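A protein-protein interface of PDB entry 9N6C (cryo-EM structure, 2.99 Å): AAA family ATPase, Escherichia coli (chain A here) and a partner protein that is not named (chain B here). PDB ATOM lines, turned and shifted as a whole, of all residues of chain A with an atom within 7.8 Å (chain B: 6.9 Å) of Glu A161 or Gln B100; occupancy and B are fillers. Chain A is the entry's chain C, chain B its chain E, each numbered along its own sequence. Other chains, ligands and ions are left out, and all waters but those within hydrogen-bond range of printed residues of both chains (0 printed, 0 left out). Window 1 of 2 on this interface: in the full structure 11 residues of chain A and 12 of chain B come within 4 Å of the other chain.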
ATOM      1  N   TRP A 101       7.995  26.658 -28.349  1.00  0.00           N
ATOM      2  CA  TRP A 101       6.949  26.327 -27.388  1.00  0.00           C
ATOM      3  C   TRP A 101       5.815  27.344 -27.451  1.00  0.00           C
ATOM      4  O   TRP A 101       4.632  26.979 -27.370  1.00  0.00           O
ATOM      5  CB  TRP A 101       7.533  26.256 -25.981  1.00  0.00           C
ATOM      6  CG  TRP A 101       8.335  25.027 -25.744  1.00  0.00           C
ATOM      7  CD1 TRP A 101       9.662  24.859 -25.985  1.00  0.00           C
ATOM      8  CD2 TRP A 101       7.865  23.789 -25.203  1.00  0.00           C
ATOM      9  NE1 TRP A 101      10.051  23.591 -25.635  1.00  0.00           N
ATOM     10  CE2 TRP A 101       8.964  22.913 -25.152  1.00  0.00           C
ATOM     11  CE3 TRP A 101       6.621  23.335 -24.759  1.00  0.00           C
ATOM     12  CZ2 TRP A 101       8.858  21.612 -24.676  1.00  0.00           C
ATOM     13  CZ3 TRP A 101       6.518  22.044 -24.287  1.00  0.00           C
ATOM     14  CH2 TRP A 101       7.629  21.197 -24.249  1.00  0.00           C
ATOM     15  N   SER A 144       8.820  34.928 -18.707  1.00  0.00           N
ATOM     16  CA  SER A 144      10.082  34.206 -18.691  1.00  0.00           C
ATOM     17  C   SER A 144       9.837  32.738 -19.003  1.00  0.00           C
ATOM     18  O   SER A 144       8.732  32.221 -18.831  1.00  0.00           O
ATOM     19  CB  SER A 144      10.789  34.339 -17.338  1.00  0.00           C
ATOM     20  OG  SER A 144       9.870  34.185 -16.274  1.00  0.00           O
ATOM     21  N   ILE A 145      10.890  32.068 -19.463  1.00  0.00           N
ATOM     22  CA  ILE A 145      10.795  30.664 -19.843  1.00  0.00           C
ATOM     23  C   ILE A 145      12.179  30.044 -19.727  1.00  0.00           C
ATOM     24  O   ILE A 145      13.192  30.672 -20.057  1.00  0.00           O
ATOM     25  CB  ILE A 145      10.207  30.514 -21.266  1.00  0.00           C
ATOM     26  CG1 ILE A 145      10.401  29.095 -21.794  1.00  0.00           C
ATOM     27  CG2 ILE A 145      10.831  31.524 -22.207  1.00  0.00           C
ATOM     28  CD1 ILE A 145       9.651  28.820 -23.071  1.00  0.00           C
ATOM     29  N   LEU A 146      12.210  28.803 -19.238  1.00  0.00           N
ATOM     30  CA  LEU A 146      13.431  28.031 -19.044  1.00  0.00           C
ATOM     31  C   LEU A 146      13.250  26.639 -19.627  1.00  0.00           C
ATOM     32  O   LEU A 146      12.244  25.976 -19.360  1.00  0.00           O
ATOM     33  CB  LEU A 146      13.784  27.932 -17.559  1.00  0.00           C
ATOM     34  CG  LEU A 146      14.877  26.936 -17.172  1.00  0.00           C
ATOM     35  CD1 LEU A 146      16.239  27.595 -17.203  1.00  0.00           C
ATOM     36  CD2 LEU A 146      14.600  26.351 -15.804  1.00  0.00           C
ATOM     37  N   ILE A 147      14.229  26.198 -20.414  1.00  0.00           N
ATOM     38  CA  ILE A 147      14.254  24.869 -21.014  1.00  0.00           C
ATOM     39  C   ILE A 147      15.545  24.190 -20.588  1.00  0.00           C
ATOM     40  O   ILE A 147      16.618  24.791 -20.680  1.00  0.00           O
ATOM     41  CB  ILE A 147      14.158  24.931 -22.550  1.00  0.00           C
ATOM     42  CG1 ILE A 147      12.928  25.728 -22.982  1.00  0.00           C
ATOM     43  CG2 ILE A 147      14.119  23.535 -23.136  1.00  0.00           C
ATOM     44  CD1 ILE A 147      11.624  25.047 -22.660  1.00  0.00           C
ATOM     45  N   THR A 148      15.459  22.942 -20.139  1.00  0.00           N
ATOM     46  CA  THR A 148      16.659  22.290 -19.640  1.00  0.00           C
ATOM     47  C   THR A 148      16.616  20.800 -19.930  1.00  0.00           C
ATOM     48  O   THR A 148      15.543  20.209 -20.067  1.00  0.00           O
ATOM     49  CB  THR A 148      16.831  22.508 -18.135  1.00  0.00           C
ATOM     50  OG1 THR A 148      17.881  21.666 -17.650  1.00  0.00           O
ATOM     51  CG2 THR A 148      15.550  22.166 -17.406  1.00  0.00           C
ATOM     52  N   SER A 157      16.888  14.607 -11.506  1.00  0.00           N
ATOM     53  CA  SER A 157      15.883  15.074 -12.447  1.00  0.00           C
ATOM     54  C   SER A 157      15.821  16.595 -12.487  1.00  0.00           C
ATOM     55  O   SER A 157      16.075  17.274 -11.490  1.00  0.00           O
ATOM     56  CB  SER A 157      14.508  14.515 -12.081  1.00  0.00           C
ATOM     57  OG  SER A 157      14.565  13.115 -11.872  1.00  0.00           O
ATOM     58  N   ARG A 158      15.478  17.121 -13.662  1.00  0.00           N
ATOM     59  CA  ARG A 158      15.225  18.541 -13.851  1.00  0.00           C
ATOM     60  C   ARG A 158      14.067  18.692 -14.826  1.00  0.00           C
ATOM     61  O   ARG A 158      13.994  17.966 -15.820  1.00  0.00           O
ATOM     62  CB  ARG A 158      16.471  19.261 -14.376  1.00  0.00           C
ATOM     63  CG  ARG A 158      17.515  19.511 -13.302  1.00  0.00           C
ATOM     64  CD  ARG A 158      18.668  20.355 -13.802  1.00  0.00           C
ATOM     65  NE  ARG A 158      18.221  21.547 -14.510  1.00  0.00           N
ATOM     66  CZ  ARG A 158      17.901  22.687 -13.915  1.00  0.00           C
ATOM     67  NH1 ARG A 158      17.946  22.817 -12.600  1.00  0.00           N
ATOM     68  NH2 ARG A 158      17.528  23.725 -14.660  1.00  0.00           N
ATOM     69  N   ASN A 159      13.167  19.629 -14.548  1.00  0.00           N
ATOM     70  CA  ASN A 159      11.986  19.843 -15.376  1.00  0.00           C
ATOM     71  C   ASN A 159      11.951  21.279 -15.899  1.00  0.00           C
ATOM     72  O   ASN A 159      12.820  22.097 -15.598  1.00  0.00           O
ATOM     73  CB  ASN A 159      10.710  19.504 -14.601  1.00  0.00           C
ATOM     74  CG  ASN A 159      10.692  20.106 -13.217  1.00  0.00           C
ATOM     75  OD1 ASN A 159      11.368  19.624 -12.311  1.00  0.00           O
ATOM     76  ND2 ASN A 159       9.910  21.163 -13.042  1.00  0.00           N
ATOM     77  N   ASN A 160      10.928  21.571 -16.697  1.00  0.00           N
ATOM     78  CA  ASN A 160      10.785  22.843 -17.390  1.00  0.00           C
ATOM     79  C   ASN A 160       9.822  23.777 -16.664  1.00  0.00           C
ATOM     80  O   ASN A 160       9.019  23.357 -15.828  1.00  0.00           O
ATOM     81  CB  ASN A 160      10.288  22.611 -18.818  1.00  0.00           C
ATOM     82  CG  ASN A 160      11.232  21.758 -19.629  1.00  0.00           C
ATOM     83  OD1 ASN A 160      12.142  21.134 -19.086  1.00  0.00           O
ATOM     84  ND2 ASN A 160      11.017  21.716 -20.936  1.00  0.00           N
ATOM     85  N   GLU A 161       9.916  25.063 -17.001  1.00  0.00           N
ATOM     86  CA  GLU A 161       9.002  26.096 -16.521  1.00  0.00           C
ATOM     87  C   GLU A 161       8.154  26.582 -17.690  1.00  0.00           C
ATOM     88  O   GLU A 161       8.695  27.082 -18.680  1.00  0.00           O
ATOM     89  CB  GLU A 161       9.773  27.256 -15.898  1.00  0.00           C
ATOM     90  CG  GLU A 161      10.745  26.840 -14.809  1.00  0.00           C
ATOM     91  CD  GLU A 161      10.080  26.060 -13.695  1.00  0.00           C
ATOM     92  OE1 GLU A 161       8.956  26.429 -13.296  1.00  0.00           O
ATOM     93  OE2 GLU A 161      10.681  25.076 -13.217  1.00  0.00           O
ATOM     94  N   LEU A 162       6.829  26.441 -17.577  1.00  0.00           N
ATOM     95  CA  LEU A 162       5.950  26.749 -18.702  1.00  0.00           C
ATOM     96  C   LEU A 162       4.705  27.552 -18.334  1.00  0.00           C
ATOM     97  O   LEU A 162       3.790  27.647 -19.160  1.00  0.00           O
ATOM     98  CB  LEU A 162       5.518  25.456 -19.404  1.00  0.00           C
ATOM     99  CG  LEU A 162       6.626  24.583 -19.993  1.00  0.00           C
ATOM    100  CD1 LEU A 162       6.112  23.184 -20.276  1.00  0.00           C
ATOM    101  CD2 LEU A 162       7.189  25.215 -21.249  1.00  0.00           C
ATOM    102  N   LEU A 163       4.629  28.129 -17.134  1.00  0.00           N
ATOM    103  CA  LEU A 163       3.435  28.879 -16.743  1.00  0.00           C
ATOM    104  C   LEU A 163       3.289  30.190 -17.514  1.00  0.00           C
ATOM    105  O   LEU A 163       2.184  30.536 -17.960  1.00  0.00           O
ATOM    106  CB  LEU A 163       3.471  29.152 -15.242  1.00  0.00           C
ATOM    107  CG  LEU A 163       2.133  29.259 -14.510  1.00  0.00           C
ATOM    108  CD1 LEU A 163       1.073  28.412 -15.191  1.00  0.00           C
ATOM    109  CD2 LEU A 163       2.291  28.852 -13.056  1.00  0.00           C
ATOM    110  N   GLY A 164       4.392  30.909 -17.722  1.00  0.00           N
ATOM    111  CA  GLY A 164       4.300  32.202 -18.381  1.00  0.00           C
ATOM    112  C   GLY A 164       3.867  32.110 -19.830  1.00  0.00           C
ATOM    113  O   GLY A 164       3.024  32.893 -20.285  1.00  0.00           O
ATOM    114  N   VAL A 165       4.411  31.146 -20.574  1.00  0.00           N
ATOM    115  CA  VAL A 165       4.087  31.113 -21.989  1.00  0.00           C
ATOM    116  C   VAL A 165       2.673  30.593 -22.191  1.00  0.00           C
ATOM    117  O   VAL A 165       1.994  30.999 -23.144  1.00  0.00           O
ATOM    118  CB  VAL A 165       5.128  30.274 -22.755  1.00  0.00           C
ATOM    119  CG1 VAL A 165       4.819  28.794 -22.649  1.00  0.00           C
ATOM    120  CG2 VAL A 165       5.190  30.707 -24.205  1.00  0.00           C
ATOM    121  N   LYS A 166       2.159  29.807 -21.243  1.00  0.00           N
ATOM    122  CA  LYS A 166       0.797  29.318 -21.385  1.00  0.00           C
ATOM    123  C   LYS A 166      -0.168  30.444 -21.064  1.00  0.00           C
ATOM    124  O   LYS A 166      -1.197  30.612 -21.738  1.00  0.00           O
ATOM    125  CB  LYS A 166       0.568  28.129 -20.455  1.00  0.00           C
ATOM    126  CG  LYS A 166       1.076  26.804 -20.987  1.00  0.00           C
ATOM    127  CD  LYS A 166       1.055  25.748 -19.899  1.00  0.00           C
ATOM    128  CE  LYS A 166       0.735  24.375 -20.455  1.00  0.00           C
ATOM    129  NZ  LYS A 166       1.970  23.609 -20.775  1.00  0.00           N
ATOM    130  N   ASP B  98      17.576  31.923  -6.498  1.00  0.00           N
ATOM    131  CA  ASP B  98      16.436  31.143  -6.034  1.00  0.00           C
ATOM    132  C   ASP B  98      16.637  29.691  -6.461  1.00  0.00           C
ATOM    133  O   ASP B  98      17.252  29.421  -7.492  1.00  0.00           O
ATOM    134  CB  ASP B  98      15.129  31.726  -6.587  1.00  0.00           C
ATOM    135  CG  ASP B  98      13.894  31.017  -6.072  1.00  0.00           C
ATOM    136  OD1 ASP B  98      12.994  31.719  -5.567  1.00  0.00           O
ATOM    137  OD2 ASP B  98      13.804  29.781  -6.160  1.00  0.00           O
ATOM    138  N   PHE B  99      16.107  28.761  -5.661  1.00  0.00           N
ATOM    139  CA  PHE B  99      16.214  27.330  -5.928  1.00  0.00           C
ATOM    140  C   PHE B  99      15.106  26.852  -6.870  1.00  0.00           C
ATOM    141  O   PHE B  99      14.396  27.646  -7.488  1.00  0.00           O
ATOM    142  CB  PHE B  99      16.182  26.537  -4.623  1.00  0.00           C
ATOM    143  CG  PHE B  99      17.414  26.692  -3.785  1.00  0.00           C
ATOM    144  CD1 PHE B  99      18.670  26.609  -4.352  1.00  0.00           C
ATOM    145  CD2 PHE B  99      17.315  26.912  -2.424  1.00  0.00           C
ATOM    146  CE1 PHE B  99      19.803  26.747  -3.577  1.00  0.00           C
ATOM    147  CE2 PHE B  99      18.444  27.052  -1.646  1.00  0.00           C
ATOM    148  CZ  PHE B  99      19.688  26.969  -2.223  1.00  0.00           C
ATOM    149  N   GLN B 100      14.970  25.533  -7.017  1.00  0.00           N
ATOM    150  CA  GLN B 100      13.949  24.941  -7.881  1.00  0.00           C
ATOM    151  C   GLN B 100      13.298  23.777  -7.148  1.00  0.00           C
ATOM    152  O   GLN B 100      13.949  22.755  -6.913  1.00  0.00           O
ATOM    153  CB  GLN B 100      14.547  24.470  -9.206  1.00  0.00           C
ATOM    154  CG  GLN B 100      13.524  24.298 -10.316  1.00  0.00           C
ATOM    155  CD  GLN B 100      13.939  23.264 -11.343  1.00  0.00           C
ATOM    156  OE1 GLN B 100      14.656  22.314 -11.031  1.00  0.00           O
ATOM    157  NE2 GLN B 100      13.486  23.442 -12.575  1.00  0.00           N
ATOM    158  N   ASN B 101      12.015  23.921  -6.811  1.00  0.00           N
ATOM    159  CA  ASN B 101      11.255  22.906  -6.081  1.00  0.00           C
ATOM    160  C   ASN B 101      11.998  22.479  -4.816  1.00  0.00           C
ATOM    161  O   ASN B 101      12.390  21.326  -4.645  1.00  0.00           O
ATOM    162  CB  ASN B 101      10.943  21.701  -6.970  1.00  0.00           C
ATOM    163  CG  ASN B 101      10.278  22.094  -8.269  1.00  0.00           C
ATOM    164  OD1 ASN B 101      10.540  21.507  -9.317  1.00  0.00           O
ATOM    165  ND2 ASN B 101       9.408  23.093  -8.208  1.00  0.00           N
ATOM    166  N   PHE B 102      12.194  23.452  -3.927  1.00  0.00           N
ATOM    167  CA  PHE B 102      13.062  23.241  -2.774  1.00  0.00           C
ATOM    168  C   PHE B 102      12.508  22.180  -1.833  1.00  0.00           C
ATOM    169  O   PHE B 102      13.255  21.331  -1.337  1.00  0.00           O
ATOM    170  CB  PHE B 102      13.265  24.562  -2.034  1.00  0.00           C
ATOM    171  CG  PHE B 102      13.964  24.419  -0.717  1.00  0.00           C
ATOM    172  CD1 PHE B 102      15.256  23.941  -0.653  1.00  0.00           C
ATOM    173  CD2 PHE B 102      13.331  24.774   0.458  1.00  0.00           C
ATOM    174  CE1 PHE B 102      15.902  23.813   0.556  1.00  0.00           C
ATOM    175  CE2 PHE B 102      13.971  24.649   1.669  1.00  0.00           C
ATOM    176  CZ  PHE B 102      15.258  24.167   1.718  1.00  0.00           C
ATOM    177  N   PHE B 103      11.200  22.207  -1.575  1.00  0.00           N
ATOM    178  CA  PHE B 103      10.645  21.409  -0.489  1.00  0.00           C
ATOM    179  C   PHE B 103      10.475  19.933  -0.822  1.00  0.00           C
ATOM    180  O   PHE B 103      10.395  19.119   0.101  1.00  0.00           O
ATOM    181  CB  PHE B 103       9.302  21.988  -0.050  1.00  0.00           C
ATOM    182  CG  PHE B 103       9.414  22.967   1.075  1.00  0.00           C
ATOM    183  CD1 PHE B 103       9.617  22.530   2.369  1.00  0.00           C
ATOM    184  CD2 PHE B 103       9.328  24.326   0.838  1.00  0.00           C
ATOM    185  CE1 PHE B 103       9.726  23.427   3.405  1.00  0.00           C
ATOM    186  CE2 PHE B 103       9.436  25.228   1.872  1.00  0.00           C
ATOM    187  CZ  PHE B 103       9.635  24.777   3.158  1.00  0.00           C
ATOM    188  N   ASN B 104      10.412  19.558  -2.096  1.00  0.00           N
ATOM    189  CA  ASN B 104      10.211  18.160  -2.456  1.00  0.00           C
ATOM    190  C   ASN B 104      11.508  17.454  -2.830  1.00  0.00           C
ATOM    191  O   ASN B 104      11.465  16.342  -3.363  1.00  0.00           O
ATOM    192  CB  ASN B 104       9.167  18.039  -3.575  1.00  0.00           C
ATOM    193  CG  ASN B 104       9.640  18.596  -4.903  1.00  0.00           C
ATOM    194  OD1 ASN B 104      10.729  18.282  -5.379  1.00  0.00           O
ATOM    195  ND2 ASN B 104       8.803  19.423  -5.517  1.00  0.00           N
ATOM    196  N   LYS B 105      12.655  18.074  -2.571  1.00  0.00           N
ATOM    197  CA  LYS B 105      13.949  17.445  -2.785  1.00  0.00           C
ATOM    198  C   LYS B 105      14.561  16.897  -1.503  1.00  0.00           C
ATOM    199  O   LYS B 105      15.702  16.429  -1.531  1.00  0.00           O
ATOM    200  CB  LYS B 105      14.919  18.436  -3.431  1.00  0.00           C
ATOM    201  CG  LYS B 105      14.489  18.920  -4.800  1.00  0.00           C
ATOM    202  CD  LYS B 105      14.035  17.771  -5.677  1.00  0.00           C
ATOM    203  CE  LYS B 105      14.359  18.033  -7.135  1.00  0.00           C
ATOM    204  NZ  LYS B 105      14.132  16.827  -7.975  1.00  0.00           N
ATOM    205  N   ASP B 186      14.015  29.560   0.696  1.00  0.00           N
ATOM    206  CA  ASP B 186      14.752  29.161  -0.495  1.00  0.00           C
ATOM    207  C   ASP B 186      15.176  30.372  -1.319  1.00  0.00           C
ATOM    208  O   ASP B 186      15.208  30.331  -2.549  1.00  0.00           O
ATOM    209  CB  ASP B 186      13.932  28.188  -1.341  1.00  0.00           C
ATOM    210  CG  ASP B 186      12.622  28.780  -1.814  1.00  0.00           C
ATOM    211  OD1 ASP B 186      12.332  29.944  -1.479  1.00  0.00           O
ATOM    212  OD2 ASP B 186      11.880  28.077  -2.531  1.00  0.00           O
ATOM    213  N   GLY B 215      21.358  16.622  -5.284  1.00  0.00           N
ATOM    214  CA  GLY B 215      19.958  16.550  -5.646  1.00  0.00           C
ATOM    215  C   GLY B 215      19.360  17.921  -5.883  1.00  0.00           C
ATOM    216  O   GLY B 215      18.532  18.099  -6.779  1.00  0.00           O
ATOM    217  N   LEU B 216      19.776  18.897  -5.082  1.00  0.00           N
ATOM    218  CA  LEU B 216      19.275  20.253  -5.222  1.00  0.00           C
ATOM    219  C   LEU B 216      19.836  20.900  -6.485  1.00  0.00           C
ATOM    220  O   LEU B 216      20.867  20.488  -7.021  1.00  0.00           O
ATOM    221  CB  LEU B 216      19.643  21.087  -3.998  1.00  0.00           C
ATOM    222  CG  LEU B 216      18.492  21.531  -3.099  1.00  0.00           C
ATOM    223  CD1 LEU B 216      18.919  22.711  -2.255  1.00  0.00           C
ATOM    224  CD2 LEU B 216      17.275  21.884  -3.927  1.00  0.00           C
ATOM    225  N   SER B 217      19.140  21.930  -6.959  1.00  0.00           N
ATOM    226  CA  SER B 217      19.547  22.614  -8.176  1.00  0.00           C
ATOM    227  C   SER B 217      19.051  24.051  -8.138  1.00  0.00           C
ATOM    228  O   SER B 217      18.161  24.403  -7.361  1.00  0.00           O
ATOM    229  CB  SER B 217      19.020  21.900  -9.424  1.00  0.00           C
ATOM    230  OG  SER B 217      19.328  22.633 -10.595  1.00  0.00           O
ATOM    231  N   ILE B 218      19.642  24.879  -8.994  1.00  0.00           N
ATOM    232  CA  ILE B 218      19.388  26.314  -9.017  1.00  0.00           C
ATOM    233  C   ILE B 218      18.505  26.642 -10.210  1.00  0.00           C
ATOM    234  O   ILE B 218      18.766  26.188 -11.330  1.00  0.00           O
ATOM    235  CB  ILE B 218      20.706  27.106  -9.076  1.00  0.00           C
ATOM    236  CG1 ILE B 218      21.275  27.305  -7.672  1.00  0.00           C
ATOM    237  CG2 ILE B 218      20.502  28.449  -9.755  1.00  0.00           C
ATOM    238  CD1 ILE B 218      20.597  28.402  -6.889  1.00  0.00           C
ATOM    239  N   ASN B 219      17.457  27.424  -9.973  1.00  0.00           N
ATOM    240  CA  ASN B 219      16.617  27.926 -11.051  1.00  0.00           C
ATOM    241  C   ASN B 219      17.334  29.096 -11.711  1.00  0.00           C
ATOM    242  O   ASN B 219      17.662  30.083 -11.045  1.00  0.00           O
ATOM    243  CB  ASN B 219      15.257  28.356 -10.511  1.00  0.00           C
ATOM    244  CG  ASN B 219      14.226  28.524 -11.600  1.00  0.00           C
ATOM    245  OD1 ASN B 219      14.560  28.747 -12.761  1.00  0.00           O
ATOM    246  ND2 ASN B 219      12.957  28.419 -11.230  1.00  0.00           N
ATOM    247  N   GLU B 220      17.569  28.996 -13.016  1.00  0.00           N
ATOM    248  CA  GLU B 220      18.376  29.985 -13.713  1.00  0.00           C
ATOM    249  C   GLU B 220      17.558  31.121 -14.305  1.00  0.00           C
ATOM    250  O   GLU B 220      18.134  32.011 -14.938  1.00  0.00           O
ATOM    251  CB  GLU B 220      19.190  29.310 -14.822  1.00  0.00           C
ATOM    252  N   SER B 221      16.241  31.119 -14.124  1.00  0.00           N
ATOM    253  CA  SER B 221      15.391  32.166 -14.671  1.00  0.00           C
ATOM    254  C   SER B 221      14.953  33.170 -13.615  1.00  0.00           C
ATOM    255  O   SER B 221      14.090  34.008 -13.893  1.00  0.00           O
ATOM    256  CB  SER B 221      14.168  31.552 -15.352  1.00  0.00           C
ATOM    257  OG  SER B 221      13.133  31.308 -14.419  1.00  0.00           O
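NH1 of Arg A158 lies within hydrogen-bond range of OG of Ser B217, 2.4 Å away. The backbone carbonyl oxygen of Asn A159 lies within hydrogen-bond range of the side-chain amide nitrogen of Gln B100 (3.4 Å). OE2 of Glu A161 lies within hydrogen-bond range of NE2 of Gln B100 (3.3 Å).
O of Leu A146 sits at hydrogen-bond distance from N of Glu A161 (3.4 Å). The side-chain hydroxyl (OG1) of Thr A148 is in hydrogen-bond range of the guanidinium group (NE) of Arg A158 (3.2 Å). The backbone NH (N) of Asn B219 is in hydrogen-bond range of the backbone carbonyl oxygen (O) of Asp B98. The backbone carbonyl oxygen (O) of Ser B217 lies within hydrogen-bond range of the backbone NH (N) of Gln B100, 3.4 Å away. OD1 of Asn B219 is in hydrogen-bond range of N of Ser B221 (3.2 Å).
Among the printed residues, pairs that only touch across the chains: Leu A146 with Asn B219 (3.9 Å), Arg A158 with Gln B100 (3.7 Å), Arg A158 with Ile B218 (3.7 Å) and Asn A159 with Asn B101 (3.6 Å).
Of the printed residues of chain B, Leu A146 touches Asn B219. Glu A161 touches one residue of chain B. Leu A162 touches none of the printed residues of chain B. Gln B100 touches three residues of chain A. Of the printed residues of chain A, Asn B101 touches Asn A159. Lys B105 touches none of the printed residues of chain A. Of the printed residues of chain A, Ile B218 touches Arg A158. The nearest residue of chain B that does not touch Glu A161 is Asn B219 (4.5 Å). The nearest printed residue of chain B that does not touch Leu A146 is Glu B220 (4.2 Å).
Of the 16 printed residues of chain B, 5 touch a printed residue of chain A. Printed residues of chain B that touch a printed residue of chain A: Gln B100, Asn B101, Ser B217, Ile B218 and Asn B219. Of the 16 printed residues of chain A, 4 touch a printed residue of chain B. Along chain A the printed residues that touch a printed residue of chain B span positions 146 to 161. Among the printed residues, 7 pairs touch across the chains. Among the printed residues, no Asp or Glu carboxylate lies within 4 Å of a Lys or Arg side-chain nitrogen of the other chain.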
